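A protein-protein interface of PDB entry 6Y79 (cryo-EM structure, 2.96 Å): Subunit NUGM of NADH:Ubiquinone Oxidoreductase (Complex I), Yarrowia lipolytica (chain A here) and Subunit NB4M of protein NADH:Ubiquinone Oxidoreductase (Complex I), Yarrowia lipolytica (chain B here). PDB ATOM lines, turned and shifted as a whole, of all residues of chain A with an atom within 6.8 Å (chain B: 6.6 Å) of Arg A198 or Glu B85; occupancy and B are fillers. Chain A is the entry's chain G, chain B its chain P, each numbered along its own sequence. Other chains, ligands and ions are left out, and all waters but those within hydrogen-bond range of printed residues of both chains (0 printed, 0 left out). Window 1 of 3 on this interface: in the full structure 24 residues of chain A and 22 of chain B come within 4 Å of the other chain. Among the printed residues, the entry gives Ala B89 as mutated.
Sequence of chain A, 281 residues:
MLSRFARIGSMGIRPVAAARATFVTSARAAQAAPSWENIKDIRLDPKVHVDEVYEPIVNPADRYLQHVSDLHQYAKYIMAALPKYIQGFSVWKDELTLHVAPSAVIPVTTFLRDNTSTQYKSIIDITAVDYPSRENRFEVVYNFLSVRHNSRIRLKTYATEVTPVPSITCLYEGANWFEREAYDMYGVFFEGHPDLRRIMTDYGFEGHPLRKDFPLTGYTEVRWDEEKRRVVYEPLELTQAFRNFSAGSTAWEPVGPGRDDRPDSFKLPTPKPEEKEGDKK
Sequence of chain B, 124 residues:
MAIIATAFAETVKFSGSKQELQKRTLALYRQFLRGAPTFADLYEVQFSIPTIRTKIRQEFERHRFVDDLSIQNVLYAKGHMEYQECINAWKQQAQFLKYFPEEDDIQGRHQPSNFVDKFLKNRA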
ATOM      1  N   ARG A 180     -27.458 -12.750  -0.813  1.00  0.00           N
ATOM      2  CA  ARG A 180     -26.249 -13.536  -0.761  1.00  0.00           C
ATOM      3  C   ARG A 180     -26.264 -14.522   0.395  1.00  0.00           C
ATOM      4  O   ARG A 180     -25.836 -15.668   0.218  1.00  0.00           O
ATOM      5  CB  ARG A 180     -25.074 -12.586  -0.675  1.00  0.00           C
ATOM      6  CG  ARG A 180     -23.797 -13.252  -0.761  1.00  0.00           C
ATOM      7  CD  ARG A 180     -22.717 -12.252  -0.744  1.00  0.00           C
ATOM      8  NE  ARG A 180     -21.452 -12.932  -0.582  1.00  0.00           N
ATOM      9  CZ  ARG A 180     -20.306 -12.304  -0.413  1.00  0.00           C
ATOM     10  NH1 ARG A 180     -20.293 -10.985  -0.384  1.00  0.00           N
ATOM     11  NH2 ARG A 180     -19.187 -12.995  -0.260  1.00  0.00           N
ATOM     12  N   TYR A 183     -28.353 -17.161  -0.573  1.00  0.00           N
ATOM     13  CA  TYR A 183     -27.637 -18.020  -1.491  1.00  0.00           C
ATOM     14  C   TYR A 183     -26.877 -19.106  -0.749  1.00  0.00           C
ATOM     15  O   TYR A 183     -26.901 -20.269  -1.150  1.00  0.00           O
ATOM     16  CB  TYR A 183     -26.679 -17.211  -2.344  1.00  0.00           C
ATOM     17  CG  TYR A 183     -25.902 -18.143  -3.197  1.00  0.00           C
ATOM     18  CD1 TYR A 183     -26.558 -18.947  -4.103  1.00  0.00           C
ATOM     19  CD2 TYR A 183     -24.531 -18.281  -3.056  1.00  0.00           C
ATOM     20  CE1 TYR A 183     -25.892 -19.832  -4.843  1.00  0.00           C
ATOM     21  CE2 TYR A 183     -23.849 -19.179  -3.814  1.00  0.00           C
ATOM     22  CZ  TYR A 183     -24.543 -19.948  -4.710  1.00  0.00           C
ATOM     23  OH  TYR A 183     -23.885 -20.847  -5.496  1.00  0.00           O
ATOM     24  N   ASP A 184     -26.167 -18.752   0.319  1.00  0.00           N
ATOM     25  CA  ASP A 184     -25.214 -19.720   0.850  1.00  0.00           C
ATOM     26  C   ASP A 184     -25.901 -20.753   1.724  1.00  0.00           C
ATOM     27  O   ASP A 184     -25.528 -21.929   1.721  1.00  0.00           O
ATOM     28  CB  ASP A 184     -24.111 -19.017   1.625  1.00  0.00           C
ATOM     29  CG  ASP A 184     -22.871 -19.864   1.742  1.00  0.00           C
ATOM     30  OD1 ASP A 184     -22.862 -21.028   1.292  1.00  0.00           O
ATOM     31  OD2 ASP A 184     -21.881 -19.372   2.275  1.00  0.00           O
ATOM     32  N   ASP A 195     -21.910 -10.081  -7.914  1.00  0.00           N
ATOM     33  CA  ASP A 195     -21.197 -10.774  -6.837  1.00  0.00           C
ATOM     34  C   ASP A 195     -22.128 -11.566  -5.940  1.00  0.00           C
ATOM     35  O   ASP A 195     -22.239 -11.321  -4.744  1.00  0.00           O
ATOM     36  CB  ASP A 195     -20.333  -9.803  -6.033  1.00  0.00           C
ATOM     37  CG  ASP A 195     -18.943  -9.671  -6.610  1.00  0.00           C
ATOM     38  OD1 ASP A 195     -18.398 -10.706  -7.035  1.00  0.00           O
ATOM     39  OD2 ASP A 195     -18.469  -8.535  -6.698  1.00  0.00           O
ATOM     40  N   LEU A 196     -22.790 -12.522  -6.552  1.00  0.00           N
ATOM     41  CA  LEU A 196     -23.322 -13.671  -5.857  1.00  0.00           C
ATOM     42  C   LEU A 196     -22.160 -14.624  -5.627  1.00  0.00           C
ATOM     43  O   LEU A 196     -21.555 -15.106  -6.589  1.00  0.00           O
ATOM     44  CB  LEU A 196     -24.410 -14.336  -6.687  1.00  0.00           C
ATOM     45  CG  LEU A 196     -25.192 -15.399  -5.955  1.00  0.00           C
ATOM     46  CD1 LEU A 196     -26.042 -14.691  -4.947  1.00  0.00           C
ATOM     47  CD2 LEU A 196     -26.023 -16.150  -6.952  1.00  0.00           C
ATOM     48  N   ARG A 197     -21.815 -14.852  -4.367  1.00  0.00           N
ATOM     49  CA  ARG A 197     -20.959 -15.959  -3.969  1.00  0.00           C
ATOM     50  C   ARG A 197     -21.285 -16.282  -2.521  1.00  0.00           C
ATOM     51  O   ARG A 197     -22.292 -15.820  -1.979  1.00  0.00           O
ATOM     52  CB  ARG A 197     -19.479 -15.634  -4.161  1.00  0.00           C
ATOM     53  CG  ARG A 197     -19.065 -14.419  -3.429  1.00  0.00           C
ATOM     54  CD  ARG A 197     -17.609 -14.122  -3.628  1.00  0.00           C
ATOM     55  NE  ARG A 197     -17.175 -13.131  -2.656  1.00  0.00           N
ATOM     56  CZ  ARG A 197     -17.387 -11.826  -2.767  1.00  0.00           C
ATOM     57  NH1 ARG A 197     -18.019 -11.326  -3.820  1.00  0.00           N
ATOM     58  NH2 ARG A 197     -16.960 -11.009  -1.821  1.00  0.00           N
ATOM     59  N   ARG A 198     -20.440 -17.080  -1.887  1.00  0.00           N
ATOM     60  CA  ARG A 198     -20.736 -17.510  -0.536  1.00  0.00           C
ATOM     61  C   ARG A 198     -20.412 -16.414   0.472  1.00  0.00           C
ATOM     62  O   ARG A 198     -19.597 -15.521   0.232  1.00  0.00           O
ATOM     63  CB  ARG A 198     -19.971 -18.787  -0.217  1.00  0.00           C
ATOM     64  CG  ARG A 198     -18.519 -18.603   0.083  1.00  0.00           C
ATOM     65  CD  ARG A 198     -17.866 -19.922   0.369  1.00  0.00           C
ATOM     66  NE  ARG A 198     -18.018 -20.896  -0.706  1.00  0.00           N
ATOM     67  CZ  ARG A 198     -18.725 -22.015  -0.598  1.00  0.00           C
ATOM     68  NH1 ARG A 198     -19.349 -22.288   0.538  1.00  0.00           N
ATOM     69  NH2 ARG A 198     -18.817 -22.853  -1.619  1.00  0.00           N
ATOM     70  N   ILE A 199     -21.099 -16.477   1.609  1.00  0.00           N
ATOM     71  CA  ILE A 199     -20.858 -15.585   2.734  1.00  0.00           C
ATOM     72  C   ILE A 199     -21.177 -16.363   4.001  1.00  0.00           C
ATOM     73  O   ILE A 199     -22.039 -17.242   4.001  1.00  0.00           O
ATOM     74  CB  ILE A 199     -21.689 -14.281   2.626  1.00  0.00           C
ATOM     75  CG1 ILE A 199     -21.224 -13.255   3.650  1.00  0.00           C
ATOM     76  CG2 ILE A 199     -23.178 -14.533   2.753  1.00  0.00           C
ATOM     77  CD1 ILE A 199     -22.024 -12.039   3.655  1.00  0.00           C
ATOM     78  N   MET A 200     -20.432 -16.069   5.069  1.00  0.00           N
ATOM     79  CA  MET A 200     -20.549 -16.690   6.398  1.00  0.00           C
ATOM     80  C   MET A 200     -20.474 -18.216   6.343  1.00  0.00           C
ATOM     81  O   MET A 200     -21.110 -18.927   7.119  1.00  0.00           O
ATOM     82  CB  MET A 200     -21.770 -16.174   7.193  1.00  0.00           C
ATOM     83  CG  MET A 200     -23.204 -16.538   6.825  1.00  0.00           C
ATOM     84  SD  MET A 200     -24.357 -15.520   7.741  1.00  0.00           S
ATOM     85  CE  MET A 200     -23.829 -13.900   7.209  1.00  0.00           C
ATOM     86  N   THR A 201     -19.648 -18.722   5.433  1.00  0.00           N
ATOM     87  CA  THR A 201     -19.258 -20.123   5.409  1.00  0.00           C
ATOM     88  C   THR A 201     -17.813 -20.190   4.927  1.00  0.00           C
ATOM     89  O   THR A 201     -17.317 -19.267   4.275  1.00  0.00           O
ATOM     90  CB  THR A 201     -20.177 -20.966   4.508  1.00  0.00           C
ATOM     91  OG1 THR A 201     -21.526 -20.508   4.620  1.00  0.00           O
ATOM     92  CG2 THR A 201     -20.194 -22.387   4.950  1.00  0.00           C
ATOM     93  N   ASP A 202     -17.133 -21.274   5.307  1.00  0.00           N
ATOM     94  CA  ASP A 202     -15.806 -21.688   4.861  1.00  0.00           C
ATOM     95  C   ASP A 202     -15.660 -21.591   3.345  1.00  0.00           C
ATOM     96  O   ASP A 202     -16.631 -21.827   2.629  1.00  0.00           O
ATOM     97  CB  ASP A 202     -15.580 -23.122   5.337  1.00  0.00           C
ATOM     98  CG  ASP A 202     -14.142 -23.543   5.290  1.00  0.00           C
ATOM     99  OD1 ASP A 202     -13.269 -22.676   5.111  1.00  0.00           O
ATOM    100  OD2 ASP A 202     -13.887 -24.757   5.434  1.00  0.00           O
ATOM    101  N   TYR A 203     -14.474 -21.241   2.839  1.00  0.00           N
ATOM    102  CA  TYR A 203     -14.347 -20.927   1.416  1.00  0.00           C
ATOM    103  C   TYR A 203     -14.443 -22.171   0.542  1.00  0.00           C
ATOM    104  O   TYR A 203     -15.034 -22.127  -0.542  1.00  0.00           O
ATOM    105  CB  TYR A 203     -13.033 -20.213   1.140  1.00  0.00           C
ATOM    106  CG  TYR A 203     -12.926 -18.832   1.718  1.00  0.00           C
ATOM    107  CD1 TYR A 203     -13.566 -17.758   1.122  1.00  0.00           C
ATOM    108  CD2 TYR A 203     -12.160 -18.598   2.846  1.00  0.00           C
ATOM    109  CE1 TYR A 203     -13.460 -16.491   1.642  1.00  0.00           C
ATOM    110  CE2 TYR A 203     -12.046 -17.335   3.374  1.00  0.00           C
ATOM    111  CZ  TYR A 203     -12.697 -16.286   2.769  1.00  0.00           C
ATOM    112  OH  TYR A 203     -12.580 -15.027   3.298  1.00  0.00           O
ATOM    113  N   GLY A 204     -13.879 -23.283   0.985  1.00  0.00           N
ATOM    114  CA  GLY A 204     -13.951 -24.488   0.187  1.00  0.00           C
ATOM    115  C   GLY A 204     -15.111 -25.378   0.568  1.00  0.00           C
ATOM    116  O   GLY A 204     -15.109 -26.572   0.263  1.00  0.00           O
ATOM    117  N   PHE A 205     -16.113 -24.802   1.229  1.00  0.00           N
ATOM    118  CA  PHE A 205     -17.228 -25.568   1.769  1.00  0.00           C
ATOM    119  C   PHE A 205     -18.137 -26.030   0.641  1.00  0.00           C
ATOM    120  O   PHE A 205     -18.705 -25.206  -0.081  1.00  0.00           O
ATOM    121  CB  PHE A 205     -17.999 -24.714   2.770  1.00  0.00           C
ATOM    122  CG  PHE A 205     -19.085 -25.441   3.500  1.00  0.00           C
ATOM    123  CD1 PHE A 205     -18.805 -26.162   4.642  1.00  0.00           C
ATOM    124  CD2 PHE A 205     -20.395 -25.374   3.065  1.00  0.00           C
ATOM    125  CE1 PHE A 205     -19.802 -26.817   5.313  1.00  0.00           C
ATOM    126  CE2 PHE A 205     -21.386 -26.022   3.738  1.00  0.00           C
ATOM    127  CZ  PHE A 205     -21.089 -26.744   4.860  1.00  0.00           C
ATOM    128  N   GLU A 206     -18.279 -27.339   0.488  1.00  0.00           N
ATOM    129  CA  GLU A 206     -19.220 -27.901  -0.466  1.00  0.00           C
ATOM    130  C   GLU A 206     -20.462 -28.337   0.297  1.00  0.00           C
ATOM    131  O   GLU A 206     -20.388 -29.202   1.176  1.00  0.00           O
ATOM    132  CB  GLU A 206     -18.613 -29.071  -1.240  1.00  0.00           C
ATOM    133  CG  GLU A 206     -19.179 -29.215  -2.651  1.00  0.00           C
ATOM    134  CD  GLU A 206     -18.908 -30.574  -3.265  1.00  0.00           C
ATOM    135  OE1 GLU A 206     -17.911 -31.211  -2.871  1.00  0.00           O
ATOM    136  OE2 GLU A 206     -19.697 -31.014  -4.128  1.00  0.00           O
ATOM    137  N   GLY A 207     -21.591 -27.732  -0.037  1.00  0.00           N
ATOM    138  CA  GLY A 207     -22.839 -27.962   0.656  1.00  0.00           C
ATOM    139  C   GLY A 207     -23.553 -26.663   0.954  1.00  0.00           C
ATOM    140  O   GLY A 207     -22.974 -25.579   0.948  1.00  0.00           O
ATOM    141  N   HIS A 208     -24.847 -26.795   1.203  1.00  0.00           N
ATOM    142  CA  HIS A 208     -25.682 -25.672   1.617  1.00  0.00           C
ATOM    143  C   HIS A 208     -26.293 -26.044   2.955  1.00  0.00           C
ATOM    144  O   HIS A 208     -27.136 -26.961   3.006  1.00  0.00           O
ATOM    145  CB  HIS A 208     -26.742 -25.356   0.572  1.00  0.00           C
ATOM    146  CG  HIS A 208     -26.169 -24.910  -0.732  1.00  0.00           C
ATOM    147  ND1 HIS A 208     -25.797 -23.607  -0.974  1.00  0.00           N
ATOM    148  CD2 HIS A 208     -25.870 -25.601  -1.855  1.00  0.00           C
ATOM    149  CE1 HIS A 208     -25.306 -23.512  -2.194  1.00  0.00           C
ATOM    150  NE2 HIS A 208     -25.340 -24.708  -2.751  1.00  0.00           N
ATOM    151  N   PHE B  39      -1.642 -18.942  -9.031  1.00  0.00           N
ATOM    152  CA  PHE B  39      -2.056 -19.850  -7.967  1.00  0.00           C
ATOM    153  C   PHE B  39      -0.853 -20.572  -7.385  1.00  0.00           C
ATOM    154  O   PHE B  39      -0.811 -20.848  -6.180  1.00  0.00           O
ATOM    155  CB  PHE B  39      -3.048 -20.889  -8.469  1.00  0.00           C
ATOM    156  CG  PHE B  39      -4.375 -20.340  -8.918  1.00  0.00           C
ATOM    157  CD1 PHE B  39      -4.787 -19.078  -8.565  1.00  0.00           C
ATOM    158  CD2 PHE B  39      -5.215 -21.116  -9.706  1.00  0.00           C
ATOM    159  CE1 PHE B  39      -5.994 -18.581  -8.994  1.00  0.00           C
ATOM    160  CE2 PHE B  39      -6.423 -20.627 -10.136  1.00  0.00           C
ATOM    161  CZ  PHE B  39      -6.815 -19.361  -9.782  1.00  0.00           C
ATOM    162  N   TYR B  43      -0.098 -19.491  -3.361  1.00  0.00           N
ATOM    163  CA  TYR B  43      -0.377 -20.439  -2.297  1.00  0.00           C
ATOM    164  C   TYR B  43       0.831 -21.255  -1.872  1.00  0.00           C
ATOM    165  O   TYR B  43       0.658 -22.193  -1.092  1.00  0.00           O
ATOM    166  CB  TYR B  43      -1.512 -21.373  -2.715  1.00  0.00           C
ATOM    167  CG  TYR B  43      -2.818 -20.642  -2.835  1.00  0.00           C
ATOM    168  CD1 TYR B  43      -3.515 -20.264  -1.708  1.00  0.00           C
ATOM    169  CD2 TYR B  43      -3.341 -20.302  -4.076  1.00  0.00           C
ATOM    170  CE1 TYR B  43      -4.693 -19.581  -1.805  1.00  0.00           C
ATOM    171  CE2 TYR B  43      -4.534 -19.617  -4.179  1.00  0.00           C
ATOM    172  CZ  TYR B  43      -5.200 -19.260  -3.036  1.00  0.00           C
ATOM    173  OH  TYR B  43      -6.383 -18.578  -3.125  1.00  0.00           O
ATOM    174  N   LYS B  78     -21.308 -21.960  -9.815  1.00  0.00           N
ATOM    175  CA  LYS B  78     -20.414 -22.448  -8.761  1.00  0.00           C
ATOM    176  C   LYS B  78     -18.953 -22.381  -9.193  1.00  0.00           C
ATOM    177  O   LYS B  78     -18.073 -22.033  -8.393  1.00  0.00           O
ATOM    178  CB  LYS B  78     -20.757 -23.887  -8.367  1.00  0.00           C
ATOM    179  CG  LYS B  78     -22.145 -24.144  -7.807  1.00  0.00           C
ATOM    180  CD  LYS B  78     -22.358 -23.654  -6.403  1.00  0.00           C
ATOM    181  CE  LYS B  78     -23.742 -24.057  -5.928  1.00  0.00           C
ATOM    182  NZ  LYS B  78     -23.879 -25.529  -5.844  1.00  0.00           N
ATOM    183  N   HIS B  80     -17.552 -20.274 -11.449  1.00  0.00           N
ATOM    184  CA  HIS B  80     -17.073 -18.897 -11.467  1.00  0.00           C
ATOM    185  C   HIS B  80     -16.857 -18.349 -10.061  1.00  0.00           C
ATOM    186  O   HIS B  80     -15.916 -17.572  -9.847  1.00  0.00           O
ATOM    187  CB  HIS B  80     -18.040 -17.998 -12.222  1.00  0.00           C
ATOM    188  CG  HIS B  80     -17.563 -16.588 -12.331  1.00  0.00           C
ATOM    189  ND1 HIS B  80     -16.593 -16.200 -13.228  1.00  0.00           N
ATOM    190  CD2 HIS B  80     -17.890 -15.479 -11.626  1.00  0.00           C
ATOM    191  CE1 HIS B  80     -16.358 -14.909 -13.087  1.00  0.00           C
ATOM    192  NE2 HIS B  80     -17.128 -14.449 -12.120  1.00  0.00           N
ATOM    193  N   MET B  81     -17.702 -18.741  -9.095  1.00  0.00           N
ATOM    194  CA  MET B  81     -17.470 -18.342  -7.707  1.00  0.00           C
ATOM    195  C   MET B  81     -16.172 -18.924  -7.187  1.00  0.00           C
ATOM    196  O   MET B  81     -15.425 -18.269  -6.449  1.00  0.00           O
ATOM    197  CB  MET B  81     -18.617 -18.802  -6.823  1.00  0.00           C
ATOM    198  CG  MET B  81     -19.891 -18.048  -7.022  1.00  0.00           C
ATOM    199  SD  MET B  81     -21.259 -18.949  -6.298  1.00  0.00           S
ATOM    200  CE  MET B  81     -22.630 -18.182  -7.138  1.00  0.00           C
ATOM    201  N   GLU B  82     -15.883 -20.155  -7.586  1.00  0.00           N
ATOM    202  CA  GLU B  82     -14.638 -20.787  -7.189  1.00  0.00           C
ATOM    203  C   GLU B  82     -13.422 -20.096  -7.780  1.00  0.00           C
ATOM    204  O   GLU B  82     -12.415 -19.890  -7.085  1.00  0.00           O
ATOM    205  CB  GLU B  82     -14.670 -22.244  -7.603  1.00  0.00           C
ATOM    206  CG  GLU B  82     -13.450 -22.960  -7.190  1.00  0.00           C
ATOM    207  CD  GLU B  82     -13.251 -22.882  -5.707  1.00  0.00           C
ATOM    208  OE1 GLU B  82     -14.239 -22.896  -4.876  1.00  0.00           O
ATOM    209  OE2 GLU B  82     -12.081 -22.879  -5.280  1.00  0.00           O
ATOM    210  N   TYR B  83     -13.523 -19.685  -9.043  1.00  0.00           N
ATOM    211  CA  TYR B  83     -12.447 -18.930  -9.670  1.00  0.00           C
ATOM    212  C   TYR B  83     -12.226 -17.595  -8.976  1.00  0.00           C
ATOM    213  O   TYR B  83     -11.082 -17.196  -8.743  1.00  0.00           O
ATOM    214  CB  TYR B  83     -12.750 -18.698 -11.143  1.00  0.00           C
ATOM    215  CG  TYR B  83     -11.657 -17.903 -11.786  1.00  0.00           C
ATOM    216  CD1 TYR B  83     -10.398 -18.449 -11.943  1.00  0.00           C
ATOM    217  CD2 TYR B  83     -11.864 -16.591 -12.189  1.00  0.00           C
ATOM    218  CE1 TYR B  83      -9.385 -17.734 -12.499  1.00  0.00           C
ATOM    219  CE2 TYR B  83     -10.851 -15.863 -12.745  1.00  0.00           C
ATOM    220  CZ  TYR B  83      -9.614 -16.442 -12.897  1.00  0.00           C
ATOM    221  OH  TYR B  83      -8.592 -15.727 -13.462  1.00  0.00           O
ATOM    222  N   GLN B  84     -13.315 -16.894  -8.644  1.00  0.00           N
ATOM    223  CA  GLN B  84     -13.207 -15.588  -7.998  1.00  0.00           C
ATOM    224  C   GLN B  84     -12.585 -15.698  -6.611  1.00  0.00           C
ATOM    225  O   GLN B  84     -11.831 -14.814  -6.192  1.00  0.00           O
ATOM    226  CB  GLN B  84     -14.583 -14.936  -7.917  1.00  0.00           C
ATOM    227  CG  GLN B  84     -14.580 -13.523  -7.388  1.00  0.00           C
ATOM    228  CD  GLN B  84     -15.969 -12.996  -7.152  1.00  0.00           C
ATOM    229  OE1 GLN B  84     -16.953 -13.693  -7.375  1.00  0.00           O
ATOM    230  NE2 GLN B  84     -16.059 -11.761  -6.686  1.00  0.00           N
ATOM    231  N   GLU B  85     -12.878 -16.783  -5.886  1.00  0.00           N
ATOM    232  CA  GLU B  85     -12.224 -16.993  -4.599  1.00  0.00           C
ATOM    233  C   GLU B  85     -10.747 -17.314  -4.763  1.00  0.00           C
ATOM    234  O   GLU B  85      -9.917 -16.832  -3.987  1.00  0.00           O
ATOM    235  CB  GLU B  85     -12.910 -18.111  -3.824  1.00  0.00           C
ATOM    236  CG  GLU B  85     -14.244 -17.732  -3.258  1.00  0.00           C
ATOM    237  CD  GLU B  85     -14.921 -18.898  -2.585  1.00  0.00           C
ATOM    238  OE1 GLU B  85     -14.313 -19.988  -2.541  1.00  0.00           O
ATOM    239  OE2 GLU B  85     -16.063 -18.728  -2.117  1.00  0.00           O
ATOM    240  N   CYS B  86     -10.398 -18.133  -5.760  1.00  0.00           N
ATOM    241  CA  CYS B  86      -9.004 -18.553  -5.915  1.00  0.00           C
ATOM    242  C   CYS B  86      -8.119 -17.429  -6.435  1.00  0.00           C
ATOM    243  O   CYS B  86      -6.954 -17.319  -6.042  1.00  0.00           O
ATOM    244  CB  CYS B  86      -8.917 -19.754  -6.847  1.00  0.00           C
ATOM    245  SG  CYS B  86      -9.386 -21.295  -6.086  1.00  0.00           S
ATOM    246  N   ILE B  87      -8.649 -16.588  -7.317  1.00  0.00           N
ATOM    247  CA  ILE B  87      -7.825 -15.564  -7.942  1.00  0.00           C
ATOM    248  C   ILE B  87      -7.619 -14.366  -7.015  1.00  0.00           C
ATOM    249  O   ILE B  87      -6.592 -13.686  -7.101  1.00  0.00           O
ATOM    250  CB  ILE B  87      -8.439 -15.159  -9.301  1.00  0.00           C
ATOM    251  CG1 ILE B  87      -7.421 -14.428 -10.160  1.00  0.00           C
ATOM    252  CG2 ILE B  87      -9.663 -14.287  -9.166  1.00  0.00           C
ATOM    253  CD1 ILE B  87      -6.256 -15.261 -10.489  1.00  0.00           C
ATOM    254  N   ASN B  88      -8.546 -14.110  -6.096  1.00  0.00           N
ATOM    255  CA  ASN B  88      -8.488 -12.906  -5.285  1.00  0.00           C
ATOM    256  C   ASN B  88      -7.681 -13.089  -4.014  1.00  0.00           C
ATOM    257  O   ASN B  88      -7.583 -12.132  -3.238  1.00  0.00           O
ATOM    258  CB  ASN B  88      -9.899 -12.446  -4.932  1.00  0.00           C
ATOM    259  CG  ASN B  88     -10.556 -11.665  -6.040  1.00  0.00           C
ATOM    260  OD1 ASN B  88      -9.912 -10.879  -6.724  1.00  0.00           O
ATOM    261  ND2 ASN B  88     -11.847 -11.872  -6.223  1.00  0.00           N
ATOM    262  N   ALA B  89      -7.110 -14.278  -3.808  1.00  0.00           N
ATOM    263  CA  ALA B  89      -6.351 -14.673  -2.619  1.00  0.00           C
ATOM    264  C   ALA B  89      -7.182 -14.486  -1.350  1.00  0.00           C
ATOM    265  O   ALA B  89      -6.820 -13.767  -0.421  1.00  0.00           O
ATOM    266  CB  ALA B  89      -5.020 -13.922  -2.525  1.00  0.00           C
ATOM    267  N   TRP B  90      -8.321 -15.165  -1.349  1.00  0.00           N
ATOM    268  CA  TRP B  90      -9.230 -15.189  -0.215  1.00  0.00           C
ATOM    269  C   TRP B  90      -9.221 -16.533   0.476  1.00  0.00           C
ATOM    270  O   TRP B  90      -9.107 -16.603   1.703  1.00  0.00           O
ATOM    271  CB  TRP B  90     -10.641 -14.883  -0.680  1.00  0.00           C
ATOM    272  CG  TRP B  90     -10.811 -13.517  -1.084  1.00  0.00           C
ATOM    273  CD1 TRP B  90      -9.981 -12.475  -0.837  1.00  0.00           C
ATOM    274  CD2 TRP B  90     -11.901 -13.005  -1.814  1.00  0.00           C
ATOM    275  NE1 TRP B  90     -10.493 -11.331  -1.379  1.00  0.00           N
ATOM    276  CE2 TRP B  90     -11.680 -11.636  -1.986  1.00  0.00           C
ATOM    277  CE3 TRP B  90     -13.052 -13.577  -2.348  1.00  0.00           C
ATOM    278  CZ2 TRP B  90     -12.566 -10.833  -2.663  1.00  0.00           C
ATOM    279  CZ3 TRP B  90     -13.923 -12.787  -3.015  1.00  0.00           C
ATOM    280  CH2 TRP B  90     -13.688 -11.432  -3.160  1.00  0.00           C
ATOM    281  N   LYS B  91      -9.385 -17.592  -0.301  1.00  0.00           N
ATOM    282  CA  LYS B  91      -9.018 -18.930   0.113  1.00  0.00           C
ATOM    283  C   LYS B  91      -7.572 -18.947   0.582  1.00  0.00           C
ATOM    284  O   LYS B  91      -6.727 -18.207   0.080  1.00  0.00           O
ATOM    285  CB  LYS B  91      -9.214 -19.866  -1.070  1.00  0.00           C
ATOM    286  CG  LYS B  91      -9.054 -21.318  -0.794  1.00  0.00           C
ATOM    287  CD  LYS B  91      -9.254 -22.043  -2.084  1.00  0.00           C
ATOM    288  CE  LYS B  91     -10.694 -21.985  -2.494  1.00  0.00           C
ATOM    289  NZ  LYS B  91     -11.511 -22.898  -1.674  1.00  0.00           N
ATOM    290  N   TYR B  99      -8.158 -29.474  -2.786  1.00  0.00           N
ATOM    291  CA  TYR B  99      -8.293 -30.038  -4.129  1.00  0.00           C
ATOM    292  C   TYR B  99      -7.315 -31.145  -4.398  1.00  0.00           C
ATOM    293  O   TYR B  99      -7.482 -31.880  -5.374  1.00  0.00           O
ATOM    294  CB  TYR B  99      -8.099 -28.962  -5.202  1.00  0.00           C
ATOM    295  CG  TYR B  99      -9.212 -27.967  -5.141  1.00  0.00           C
ATOM    296  CD1 TYR B  99     -10.416 -28.362  -4.644  1.00  0.00           C
ATOM    297  CD2 TYR B  99      -9.056 -26.653  -5.520  1.00  0.00           C
ATOM    298  CE1 TYR B  99     -11.442 -27.543  -4.499  1.00  0.00           C
ATOM    299  CE2 TYR B  99     -10.113 -25.759  -5.409  1.00  0.00           C
ATOM    300  CZ  TYR B  99     -11.320 -26.258  -4.885  1.00  0.00           C
ATOM    301  OH  TYR B  99     -12.463 -25.556  -4.685  1.00  0.00           O
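SD of Met B81 sits at hydrogen-bond distance from OH of Tyr A183, 3.3 Å away. The backbone carbonyl oxygen of Tyr A203 sits close to the side-chain carboxylate of Glu B85 (3.0 Å). OE2 of Glu B85 lies within salt-bridge range of NE of Arg A198, at 3.2 Å. The side-chain amide nitrogen (NE2) of Gln B84 sits at hydrogen-bond distance from the side-chain carboxylate (OD1) of Asp A195 (2.6 Å). The side-chain amide nitrogen of Gln B84 lies close to the guanidinium group of Arg A197.
The backbone carbonyl oxygen (O) of Gln B84 sits at hydrogen-bond distance from the side-chain amide nitrogen (ND2) of Asn B88. The backbone carbonyl oxygen of Asp A184 sits at hydrogen-bond distance from a ring nitrogen (ND1) of His A208. OD1 of Asp A195 lies within salt-bridge range of NH1 of Arg A197 (3.3 Å). O of Tyr A203 sits at hydrogen-bond distance from NE of Arg A198. NH1 of Arg A198 lies within salt-bridge range of OD1 of Asp A184 (3.8 Å). The side-chain hydroxyl of Tyr B43 sits close to the backbone carbonyl oxygen of Lys B91 (3.2 Å).
CE of Lys B78 touches OH of Tyr A183 (3.2 Å). Leu A196 touches Met B81. CG of Met B81 touches CB of Arg A197, 3.8 Å away. Arg A197 touches Trp B90 (NE to CZ3, 3.3 Å). Tyr A203 touches Trp B90. Tyr A203 touches Lys B91 (C to NZ, 3.7 Å). NZ of Lys B91 touches CA of Gly A204, 3.5 Å away. Lys B78 touches His A208 (NZ to NE2, 3.5 Å).
Arg A198 touches just one residue of chain B: Glu B85 (3.2 Å). Of chain A, only Arg A198 (3.2 Å) and Tyr A203 (3.0 Å) come within 4 Å of Glu B85. Of the printed residues of chain B, Arg A197 touches Met B81, Gln B84 and Trp B90. Of the printed residues of chain B, Tyr A203 touches Glu B85 (3.0 Å), Trp B90 (3.5 Å) and Lys B91 (3.7 Å). The nearest residue of chain B that does not touch Arg A198 is Met B81 (4.9 Å). The nearest residue of chain A that does not touch Glu B85 is Gly A204 (4.8 Å). The nearest printed residue of chain B that does not touch Tyr A183 is Glu B85 (8.0 Å).
Of the 17 printed residues of chain A, 8 touch a printed residue of chain B. Hydrophobic or aromatic side chains of chain A within 4 Å of the printed part of chain B: Tyr A183, Leu A196, Tyr A203 and His A208. Printed residues of chain B that touch a printed residue of chain A: Lys B78, Met B81, Gln B84, Glu B85, Trp B90 and Lys B91. Hydrophobic or aromatic side chains of chain B within 4 Å of the printed part of chain A: Met B81 and Trp B90. Among the printed residues, 13 pairs touch across the chains.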
